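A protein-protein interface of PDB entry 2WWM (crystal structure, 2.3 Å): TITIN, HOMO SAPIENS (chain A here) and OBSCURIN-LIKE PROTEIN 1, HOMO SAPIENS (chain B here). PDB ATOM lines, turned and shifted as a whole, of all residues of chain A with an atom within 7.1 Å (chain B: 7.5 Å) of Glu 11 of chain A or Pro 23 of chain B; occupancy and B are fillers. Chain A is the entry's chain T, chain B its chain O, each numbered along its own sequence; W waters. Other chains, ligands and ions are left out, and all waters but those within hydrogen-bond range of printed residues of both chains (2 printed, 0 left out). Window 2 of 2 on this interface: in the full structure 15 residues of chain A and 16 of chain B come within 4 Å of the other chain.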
ATOM      1  N   LYS A   9       2.987   3.531 -19.138  1.00  0.00           N
ATOM      2  CA  LYS A   9       4.090   2.773 -19.685  1.00  0.00           C
ATOM      3  C   LYS A   9       3.677   1.307 -19.749  1.00  0.00           C
ATOM      4  O   LYS A   9       3.398   0.688 -18.730  1.00  0.00           O
ATOM      5  CB  LYS A   9       5.352   2.982 -18.836  1.00  0.00           C
ATOM      6  CG  LYS A   9       6.601   2.205 -19.304  1.00  0.00           C
ATOM      7  CD  LYS A   9       7.131   2.685 -20.685  1.00  0.00           C
ATOM      8  CE  LYS A   9       8.552   2.152 -21.001  1.00  0.00           C
ATOM      9  NZ  LYS A   9       8.599   0.673 -21.282  1.00  0.00           N
ATOM     10  N   ILE A  10       3.608   0.773 -20.964  1.00  0.00           N
ATOM     11  CA  ILE A  10       3.340  -0.636 -21.184  1.00  0.00           C
ATOM     12  C   ILE A  10       4.601  -1.397 -20.800  1.00  0.00           C
ATOM     13  O   ILE A  10       5.704  -1.044 -21.222  1.00  0.00           O
ATOM     14  CB  ILE A  10       2.987  -0.933 -22.659  1.00  0.00           C
ATOM     15  CG1 ILE A  10       1.695  -0.229 -23.072  1.00  0.00           C
ATOM     16  CG2 ILE A  10       2.830  -2.398 -22.886  1.00  0.00           C
ATOM     17  CD1 ILE A  10       1.383  -0.341 -24.543  1.00  0.00           C
ATOM     18  N   GLU A  11       4.446  -2.415 -19.969  1.00  0.00           N
ATOM     19  CA  GLU A  11       5.546  -3.312 -19.674  1.00  0.00           C
ATOM     20  C   GLU A  11       5.457  -4.399 -20.733  1.00  0.00           C
ATOM     21  O   GLU A  11       4.590  -4.337 -21.619  1.00  0.00           O
ATOM     22  CB  GLU A  11       5.444  -3.814 -18.237  1.00  0.00           C
ATOM     23  CG  GLU A  11       5.443  -2.647 -17.250  1.00  0.00           C
ATOM     24  CD  GLU A  11       5.419  -3.058 -15.792  1.00  0.00           C
ATOM     25  OE1 GLU A  11       5.264  -4.263 -15.513  1.00  0.00           O
ATOM     26  OE2 GLU A  11       5.552  -2.170 -14.910  1.00  0.00           O
ATOM     27  N   ALA A  12       6.338  -5.374 -20.679  1.00  0.00           N
ATOM     28  CA  ALA A  12       6.446  -6.382 -21.743  1.00  0.00           C
ATOM     29  C   ALA A  12       5.120  -6.736 -22.446  1.00  0.00           C
ATOM     30  O   ALA A  12       4.113  -7.007 -21.797  1.00  0.00           O
ATOM     31  CB  ALA A  12       7.089  -7.633 -21.187  1.00  0.00           C
ATOM     32  N   LEU A  13       5.136  -6.710 -23.776  1.00  0.00           N
ATOM     33  CA  LEU A  13       4.083  -7.296 -24.606  1.00  0.00           C
ATOM     34  C   LEU A  13       4.812  -8.173 -25.611  1.00  0.00           C
ATOM     35  O   LEU A  13       5.834  -7.755 -26.132  1.00  0.00           O
ATOM     36  CB  LEU A  13       3.273  -6.217 -25.333  1.00  0.00           C
ATOM     37  CG  LEU A  13       2.097  -6.666 -26.221  1.00  0.00           C
ATOM     38  CD1 LEU A  13       0.982  -7.285 -25.402  1.00  0.00           C
ATOM     39  CD2 LEU A  13       1.541  -5.492 -27.094  1.00  0.00           C
ATOM     40  N   PRO A  14       4.317  -9.396 -25.870  1.00  0.00           N
ATOM     41  CA  PRO A  14       4.973 -10.260 -26.865  1.00  0.00           C
ATOM     42  C   PRO A  14       5.012  -9.637 -28.265  1.00  0.00           C
ATOM     43  O   PRO A  14       4.168  -8.808 -28.588  1.00  0.00           O
ATOM     44  CB  PRO A  14       4.088 -11.518 -26.879  1.00  0.00           C
ATOM     45  CG  PRO A  14       3.467 -11.548 -25.551  1.00  0.00           C
ATOM     46  CD  PRO A  14       3.237 -10.110 -25.165  1.00  0.00           C
ATOM     47  N   CYS A  29      -1.292  -8.143 -20.332  1.00  0.00           N
ATOM     48  CA  CYS A  29      -0.242  -7.136 -20.358  1.00  0.00           C
ATOM     49  C   CYS A  29      -0.349  -6.183 -19.173  1.00  0.00           C
ATOM     50  O   CYS A  29      -1.417  -5.612 -18.907  1.00  0.00           O
ATOM     51  CB  CYS A  29      -0.259  -6.338 -21.659  1.00  0.00           C
ATOM     52  SG  CYS A  29       1.279  -5.338 -21.883  1.00  0.00           S
ATOM     53  N   ALA A  30       0.779  -6.016 -18.485  1.00  0.00           N
ATOM     54  CA  ALA A  30       0.868  -5.146 -17.327  1.00  0.00           C
ATOM     55  C   ALA A  30       1.209  -3.754 -17.791  1.00  0.00           C
ATOM     56  O   ALA A  30       1.747  -3.581 -18.895  1.00  0.00           O
ATOM     57  CB  ALA A  30       1.932  -5.653 -16.356  1.00  0.00           C
ATOM     58  N   PHE A  31       0.890  -2.774 -16.947  1.00  0.00           N
ATOM     59  CA  PHE A  31       1.202  -1.368 -17.200  1.00  0.00           C
ATOM     60  C   PHE A  31       1.173  -0.531 -15.925  1.00  0.00           C
ATOM     61  O   PHE A  31       0.612  -0.949 -14.913  1.00  0.00           O
ATOM     62  CB  PHE A  31       0.227  -0.751 -18.205  1.00  0.00           C
ATOM     63  CG  PHE A  31      -1.218  -0.899 -17.835  1.00  0.00           C
ATOM     64  CD1 PHE A  31      -1.838   0.010 -17.000  1.00  0.00           C
ATOM     65  CD2 PHE A  31      -1.978  -1.949 -18.350  1.00  0.00           C
ATOM     66  CE1 PHE A  31      -3.185  -0.137 -16.675  1.00  0.00           C
ATOM     67  CE2 PHE A  31      -3.322  -2.090 -18.024  1.00  0.00           C
ATOM     68  CZ  PHE A  31      -3.913  -1.191 -17.187  1.00  0.00           C
ATOM     69  N   THR A  32       1.758   0.657 -16.002  1.00  0.00           N
ATOM     70  CA  THR A  32       1.728   1.625 -14.923  1.00  0.00           C
ATOM     71  C   THR A  32       1.212   2.939 -15.475  1.00  0.00           C
ATOM     72  O   THR A  32       1.041   3.080 -16.682  1.00  0.00           O
ATOM     73  CB  THR A  32       3.121   1.869 -14.352  1.00  0.00           C
ATOM     74  OG1 THR A  32       3.998   2.239 -15.418  1.00  0.00           O
ATOM     75  CG2 THR A  32       3.643   0.626 -13.632  1.00  0.00           C
ATOM     76  N   ASP A  63      -3.539  -2.102 -13.170  1.00  0.00           N
ATOM     77  CA  ASP A  63      -2.208  -2.343 -13.720  1.00  0.00           C
ATOM     78  C   ASP A  63      -2.143  -3.538 -14.696  1.00  0.00           C
ATOM     79  O   ASP A  63      -1.065  -4.075 -14.965  1.00  0.00           O
ATOM     80  CB  ASP A  63      -1.229  -2.534 -12.557  1.00  0.00           C
ATOM     81  CG  ASP A  63      -1.678  -3.606 -11.596  1.00  0.00           C
ATOM     82  OD1 ASP A  63      -2.128  -4.665 -12.064  1.00  0.00           O
ATOM     83  OD2 ASP A  63      -1.593  -3.399 -10.373  1.00  0.00           O
ATOM     84  N   LEU A  82      -2.053  -2.404 -28.439  1.00  0.00           N
ATOM     85  CA  LEU A  82      -2.494  -1.981 -27.123  1.00  0.00           C
ATOM     86  C   LEU A  82      -2.017  -0.551 -26.961  1.00  0.00           C
ATOM     87  O   LEU A  82      -0.826  -0.290 -27.096  1.00  0.00           O
ATOM     88  CB  LEU A  82      -1.866  -2.845 -26.035  1.00  0.00           C
ATOM     89  CG  LEU A  82      -2.028  -2.369 -24.588  1.00  0.00           C
ATOM     90  CD1 LEU A  82      -3.503  -2.139 -24.287  1.00  0.00           C
ATOM     91  CD2 LEU A  82      -1.368  -3.354 -23.593  1.00  0.00           C
ATOM     92  N   LEU A  84      -2.395   3.005 -24.410  1.00  0.00           N
ATOM     93  CA  LEU A  84      -2.745   3.522 -23.104  1.00  0.00           C
ATOM     94  C   LEU A  84      -2.754   5.039 -23.135  1.00  0.00           C
ATOM     95  O   LEU A  84      -1.947   5.657 -23.820  1.00  0.00           O
ATOM     96  CB  LEU A  84      -1.713   3.084 -22.071  1.00  0.00           C
ATOM     97  CG  LEU A  84      -1.495   1.608 -21.759  1.00  0.00           C
ATOM     98  CD1 LEU A  84      -0.448   1.518 -20.641  1.00  0.00           C
ATOM     99  CD2 LEU A  84      -2.788   0.904 -21.362  1.00  0.00           C
ATOM    100  N   ASP A  91       1.138   5.619 -24.439  1.00  0.00           N
ATOM    101  CA  ASP A  91       2.080   4.579 -24.873  1.00  0.00           C
ATOM    102  C   ASP A  91       1.339   3.560 -25.716  1.00  0.00           C
ATOM    103  O   ASP A  91       0.119   3.422 -25.606  1.00  0.00           O
ATOM    104  CB  ASP A  91       2.728   3.881 -23.668  1.00  0.00           C
ATOM    105  CG  ASP A  91       4.011   3.130 -24.029  1.00  0.00           C
ATOM    106  OD1 ASP A  91       4.497   3.220 -25.186  1.00  0.00           O
ATOM    107  OD2 ASP A  91       4.556   2.450 -23.136  1.00  0.00           O
ATOM    108  N   ALA A  93       2.063  -0.502 -27.906  1.00  0.00           N
ATOM    109  CA  ALA A  93       2.864  -1.634 -28.339  1.00  0.00           C
ATOM    110  C   ALA A  93       1.995  -2.520 -29.234  1.00  0.00           C
ATOM    111  O   ALA A  93       0.763  -2.587 -29.069  1.00  0.00           O
ATOM    112  CB  ALA A  93       3.369  -2.410 -27.156  1.00  0.00           C
ATOM    113  N   PHE B  20       0.588 -13.284 -12.855  1.00  0.00           N
ATOM    114  CA  PHE B  20       1.234 -12.853 -14.076  1.00  0.00           C
ATOM    115  C   PHE B  20       2.723 -12.715 -13.747  1.00  0.00           C
ATOM    116  O   PHE B  20       3.059 -12.440 -12.596  1.00  0.00           O
ATOM    117  CB  PHE B  20       0.589 -11.522 -14.494  1.00  0.00           C
ATOM    118  CG  PHE B  20       1.086 -10.960 -15.799  1.00  0.00           C
ATOM    119  CD1 PHE B  20       0.415 -11.212 -16.986  1.00  0.00           C
ATOM    120  CD2 PHE B  20       2.213 -10.140 -15.836  1.00  0.00           C
ATOM    121  CE1 PHE B  20       0.881 -10.673 -18.195  1.00  0.00           C
ATOM    122  CE2 PHE B  20       2.679  -9.609 -17.029  1.00  0.00           C
ATOM    123  CZ  PHE B  20       2.017  -9.871 -18.213  1.00  0.00           C
ATOM    124  N   PRO B  21       3.623 -12.949 -14.733  1.00  0.00           N
ATOM    125  CA  PRO B  21       5.065 -12.758 -14.493  1.00  0.00           C
ATOM    126  C   PRO B  21       5.482 -11.296 -14.374  1.00  0.00           C
ATOM    127  O   PRO B  21       5.092 -10.471 -15.192  1.00  0.00           O
ATOM    128  CB  PRO B  21       5.730 -13.402 -15.727  1.00  0.00           C
ATOM    129  CG  PRO B  21       4.697 -13.409 -16.772  1.00  0.00           C
ATOM    130  CD  PRO B  21       3.371 -13.553 -16.053  1.00  0.00           C
ATOM    131  N   ARG B  22       6.304 -10.991 -13.377  1.00  0.00           N
ATOM    132  CA  ARG B  22       6.696  -9.609 -13.104  1.00  0.00           C
ATOM    133  C   ARG B  22       8.111  -9.300 -13.622  1.00  0.00           C
ATOM    134  O   ARG B  22       8.945 -10.194 -13.727  1.00  0.00           O
ATOM    135  CB  ARG B  22       6.596  -9.321 -11.604  1.00  0.00           C
ATOM    136  CG  ARG B  22       5.154  -9.407 -11.031  1.00  0.00           C
ATOM    137  CD  ARG B  22       4.242  -8.239 -11.484  1.00  0.00           C
ATOM    138  NE  ARG B  22       2.822  -8.576 -11.357  1.00  0.00           N
ATOM    139  CZ  ARG B  22       1.805  -7.841 -11.818  1.00  0.00           C
ATOM    140  NH1 ARG B  22       0.556  -8.261 -11.629  1.00  0.00           N
ATOM    141  NH2 ARG B  22       2.014  -6.690 -12.458  1.00  0.00           N
ATOM    142  N   PRO B  23       8.372  -8.028 -13.965  1.00  0.00           N
ATOM    143  CA  PRO B  23       9.704  -7.629 -14.385  1.00  0.00           C
ATOM    144  C   PRO B  23      10.763  -7.846 -13.315  1.00  0.00           C
ATOM    145  O   PRO B  23      10.470  -7.738 -12.125  1.00  0.00           O
ATOM    146  CB  PRO B  23       9.555  -6.129 -14.680  1.00  0.00           C
ATOM    147  CG  PRO B  23       8.213  -5.742 -14.171  1.00  0.00           C
ATOM    148  CD  PRO B  23       7.387  -6.958 -14.188  1.00  0.00           C
ATOM    149  N   VAL B  24      11.979  -8.182 -13.733  1.00  0.00           N
ATOM    150  CA  VAL B  24      13.088  -8.266 -12.792  1.00  0.00           C
ATOM    151  C   VAL B  24      14.256  -7.400 -13.247  1.00  0.00           C
ATOM    152  O   VAL B  24      14.582  -7.317 -14.429  1.00  0.00           O
ATOM    153  CB  VAL B  24      13.557  -9.722 -12.543  1.00  0.00           C
ATOM    154  CG1 VAL B  24      12.394 -10.566 -12.072  1.00  0.00           C
ATOM    155  CG2 VAL B  24      14.160 -10.304 -13.774  1.00  0.00           C
ATOM    156  N   ARG B  25      14.861  -6.767 -12.260  1.00  0.00           N
ATOM    157  CA  ARG B  25      15.967  -5.846 -12.400  1.00  0.00           C
ATOM    158  C   ARG B  25      17.042  -6.478 -11.531  1.00  0.00           C
ATOM    159  O   ARG B  25      16.820  -6.684 -10.334  1.00  0.00           O
ATOM    160  CB  ARG B  25      15.518  -4.516 -11.810  1.00  0.00           C
ATOM    161  CG  ARG B  25      16.289  -3.291 -12.159  1.00  0.00           C
ATOM    162  CD  ARG B  25      15.519  -2.030 -11.645  1.00  0.00           C
ATOM    163  NE  ARG B  25      15.192  -2.071 -10.203  1.00  0.00           N
ATOM    164  CZ  ARG B  25      14.523  -1.111  -9.555  1.00  0.00           C
ATOM    165  NH1 ARG B  25      14.119  -0.016 -10.197  1.00  0.00           N
ATOM    166  NH2 ARG B  25      14.270  -1.221  -8.249  1.00  0.00           N
ATOM    167  N   GLU B  33      14.877 -14.707 -11.611  1.00  0.00           N
ATOM    168  CA  GLU B  33      13.797 -15.645 -11.865  1.00  0.00           C
ATOM    169  C   GLU B  33      12.543 -14.928 -12.287  1.00  0.00           C
ATOM    170  O   GLU B  33      12.254 -13.850 -11.787  1.00  0.00           O
ATOM    171  CB  GLU B  33      13.491 -16.461 -10.622  1.00  0.00           C
ATOM    172  CG  GLU B  33      12.796 -17.781 -10.937  1.00  0.00           C
ATOM    173  CD  GLU B  33      12.305 -18.503  -9.700  1.00  0.00           C
ATOM    174  OE1 GLU B  33      12.753 -18.126  -8.585  1.00  0.00           O
ATOM    175  OE2 GLU B  33      11.464 -19.437  -9.848  1.00  0.00           O
ATOM    176  N   LEU B  34      11.821 -15.522 -13.229  1.00  0.00           N
ATOM    177  CA  LEU B  34      10.439 -15.142 -13.500  1.00  0.00           C
ATOM    178  C   LEU B  34       9.558 -16.247 -12.952  1.00  0.00           C
ATOM    179  O   LEU B  34       9.924 -17.417 -13.017  1.00  0.00           O
ATOM    180  CB  LEU B  34      10.190 -14.937 -14.998  1.00  0.00           C
ATOM    181  CG  LEU B  34      11.093 -13.905 -15.685  1.00  0.00           C
ATOM    182  CD1 LEU B  34      10.872 -13.916 -17.216  1.00  0.00           C
ATOM    183  CD2 LEU B  34      10.866 -12.507 -15.118  1.00  0.00           C
ATOM    184  N   VAL B  84      12.935  -9.328 -23.221  1.00  0.00           N
ATOM    185  CA  VAL B  84      11.536  -9.686 -22.979  1.00  0.00           C
ATOM    186  C   VAL B  84      11.385 -11.184 -23.161  1.00  0.00           C
ATOM    187  O   VAL B  84      11.660 -11.720 -24.224  1.00  0.00           O
ATOM    188  CB  VAL B  84      10.579  -8.978 -23.958  1.00  0.00           C
ATOM    189  CG1 VAL B  84       9.132  -9.341 -23.640  1.00  0.00           C
ATOM    190  CG2 VAL B  84      10.764  -7.474 -23.901  1.00  0.00           C
ATOM    191  N   ALA B  99       4.134 -11.576 -20.927  1.00  0.00           N
ATOM    192  CA  ALA B  99       5.551 -11.227 -21.052  1.00  0.00           C
ATOM    193  C   ALA B  99       6.104 -10.540 -19.795  1.00  0.00           C
ATOM    194  O   ALA B  99       5.344  -9.972 -19.002  1.00  0.00           O
ATOM    195  CB  ALA B  99       5.759 -10.352 -22.257  1.00  0.00           C
ATOM    196  N   ALA B 100       7.428 -10.624 -19.611  1.00  0.00           N
ATOM    197  CA  ALA B 100       8.135  -9.791 -18.635  1.00  0.00           C
ATOM    198  C   ALA B 100       9.589  -9.468 -19.046  1.00  0.00           C
ATOM    199  O   ALA B 100      10.306 -10.287 -19.639  1.00  0.00           O
ATOM    200  CB  ALA B 100       8.095 -10.430 -17.263  1.00  0.00           C
ATOM    201  N   ALA B 101      10.004  -8.252 -18.722  1.00  0.00           N
ATOM    202  CA  ALA B 101      11.342  -7.779 -19.010  1.00  0.00           C
ATOM    203  C   ALA B 101      12.298  -8.217 -17.917  1.00  0.00           C
ATOM    204  O   ALA B 101      12.034  -8.037 -16.727  1.00  0.00           O
ATOM    205  CB  ALA B 101      11.349  -6.257 -19.139  1.00  0.00           C
ATOM    206  N   VAL B 102      13.396  -8.837 -18.330  1.00  0.00           N
ATOM    207  CA  VAL B 102      14.550  -9.005 -17.469  1.00  0.00           C
ATOM    208  C   VAL B 102      15.540  -7.914 -17.819  1.00  0.00           C
ATOM    209  O   VAL B 102      15.998  -7.842 -18.944  1.00  0.00           O
ATOM    210  CB  VAL B 102      15.180 -10.399 -17.632  1.00  0.00           C
ATOM    211  CG1 VAL B 102      16.446 -10.519 -16.811  1.00  0.00           C
ATOM    212  CG2 VAL B 102      14.154 -11.478 -17.226  1.00  0.00           C
ATOM    213  N   THR B 103      15.844  -7.051 -16.856  1.00  0.00           N
ATOM    214  CA  THR B 103      16.854  -6.006 -17.037  1.00  0.00           C
ATOM    215  C   THR B 103      18.122  -6.401 -16.272  1.00  0.00           C
ATOM    216  O   THR B 103      18.054  -6.817 -15.119  1.00  0.00           O
ATOM    217  CB  THR B 103      16.349  -4.649 -16.525  1.00  0.00           C
ATOM    218  OG1 THR B 103      15.131  -4.315 -17.198  1.00  0.00           O
ATOM    219  CG2 THR B 103      17.375  -3.559 -16.777  1.00  0.00           C
HETATM  220  O   HOH W   1       3.504  -7.007 -19.220  1.00  0.00           O
HETATM  221  O   HOH W   2       2.279  -9.429 -21.802  1.00  0.00           O
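Of the 14 printed residues of chain B, 6 touch a printed residue of chain A. Along chain B the printed residues that touch a printed residue of chain A span positions 20 to 101. Hydrophobic or aromatic side chains of chain A that line the printed part of chain B: Ala 12 and Pro 14. Along chain A the printed residues that touch a printed residue of chain B span positions 11 to 29. Among the printed residues, no Asp or Glu carboxylate lies within 4 Å of a Lys or Arg side-chain nitrogen of the other chain.
Water W1 lies within hydrogen-bond range of the backbone carbonyl oxygen of Ala 12 of chain A (2.6 Å), the backbone NH of Ala 30 of chain A (3.0 Å) and the backbone carbonyl oxygen of Ala 99 of chain B (3.5 Å). Water W2 lies within hydrogen-bond range of the backbone NH of Ala 99 of chain B (3.0 Å) and the backbone carbonyl oxygen of Ala 12 of chain A (3.0 Å).
Of the printed residues of chain B, Glu 11 of chain A touches Pro 23. Printed residues of chain A within 4 Å of Pro 23 of chain B: Glu 11. Of the printed residues of chain B, Ala 12 of chain A touches Val 84 (3.6 Å), Ala 99 (3.2 Å), Ala 100 (3.4 Å) and Ala 101 (3.9 Å). Printed residues of chain A within 4 Å of Ala 101 of chain B: Ala 12 (3.9 Å). Of the printed residues of chain A, Ala 99 of chain B touches Ala 12, Leu 13 and Pro 14. Printed residues of chain A within 4 Å of Val 84 of chain B: Ala 12. Of the printed residues of chain A, Phe 20 of chain B touches Cys 29. The nearest residue of chain B that does not touch Glu 11 of chain A is Arg 22 of chain B (5.1 Å). The nearest residue of chain A that does not touch Pro 23 of chain B is Ala 30 of chain A (6.0 Å).
The backbone NH (N) of Val 24 of chain B is in hydrogen-bond range of the backbone carbonyl oxygen (O) of Ala 101 of chain B, 3.0 Å away. The backbone carbonyl oxygen (O) of Glu 11 of chain A sits at hydrogen-bond distance from the side-chain sulfur (SG) of Cys 29 of chain A (3.5 Å). N of Glu 11 of chain A lies within hydrogen-bond range of O of Ala 30 of chain A (3.1 Å). SG of Cys 29 of chain A is in hydrogen-bond range of O of Ala 12 of chain A (3.3 Å).
Glu 11 of chain A touches Pro 23 of chain B. Ala 12 of chain A touches Val 84 of chain B. Ala 12 of chain A touches Ala 99 of chain B (CB to CB, 3.2 Å). Ala 100 of chain B touches Ala 12 of chain A (N to CB, 3.4 Å). Ala 12 of chain A touches Ala 101 of chain B. Leu 13 of chain A touches Ala 99 of chain B. Pro 14 of chain A touches Ala 99 of chain B (CD to CB, 3.9 Å). Cys 29 of chain A touches Phe 20 of chain B.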
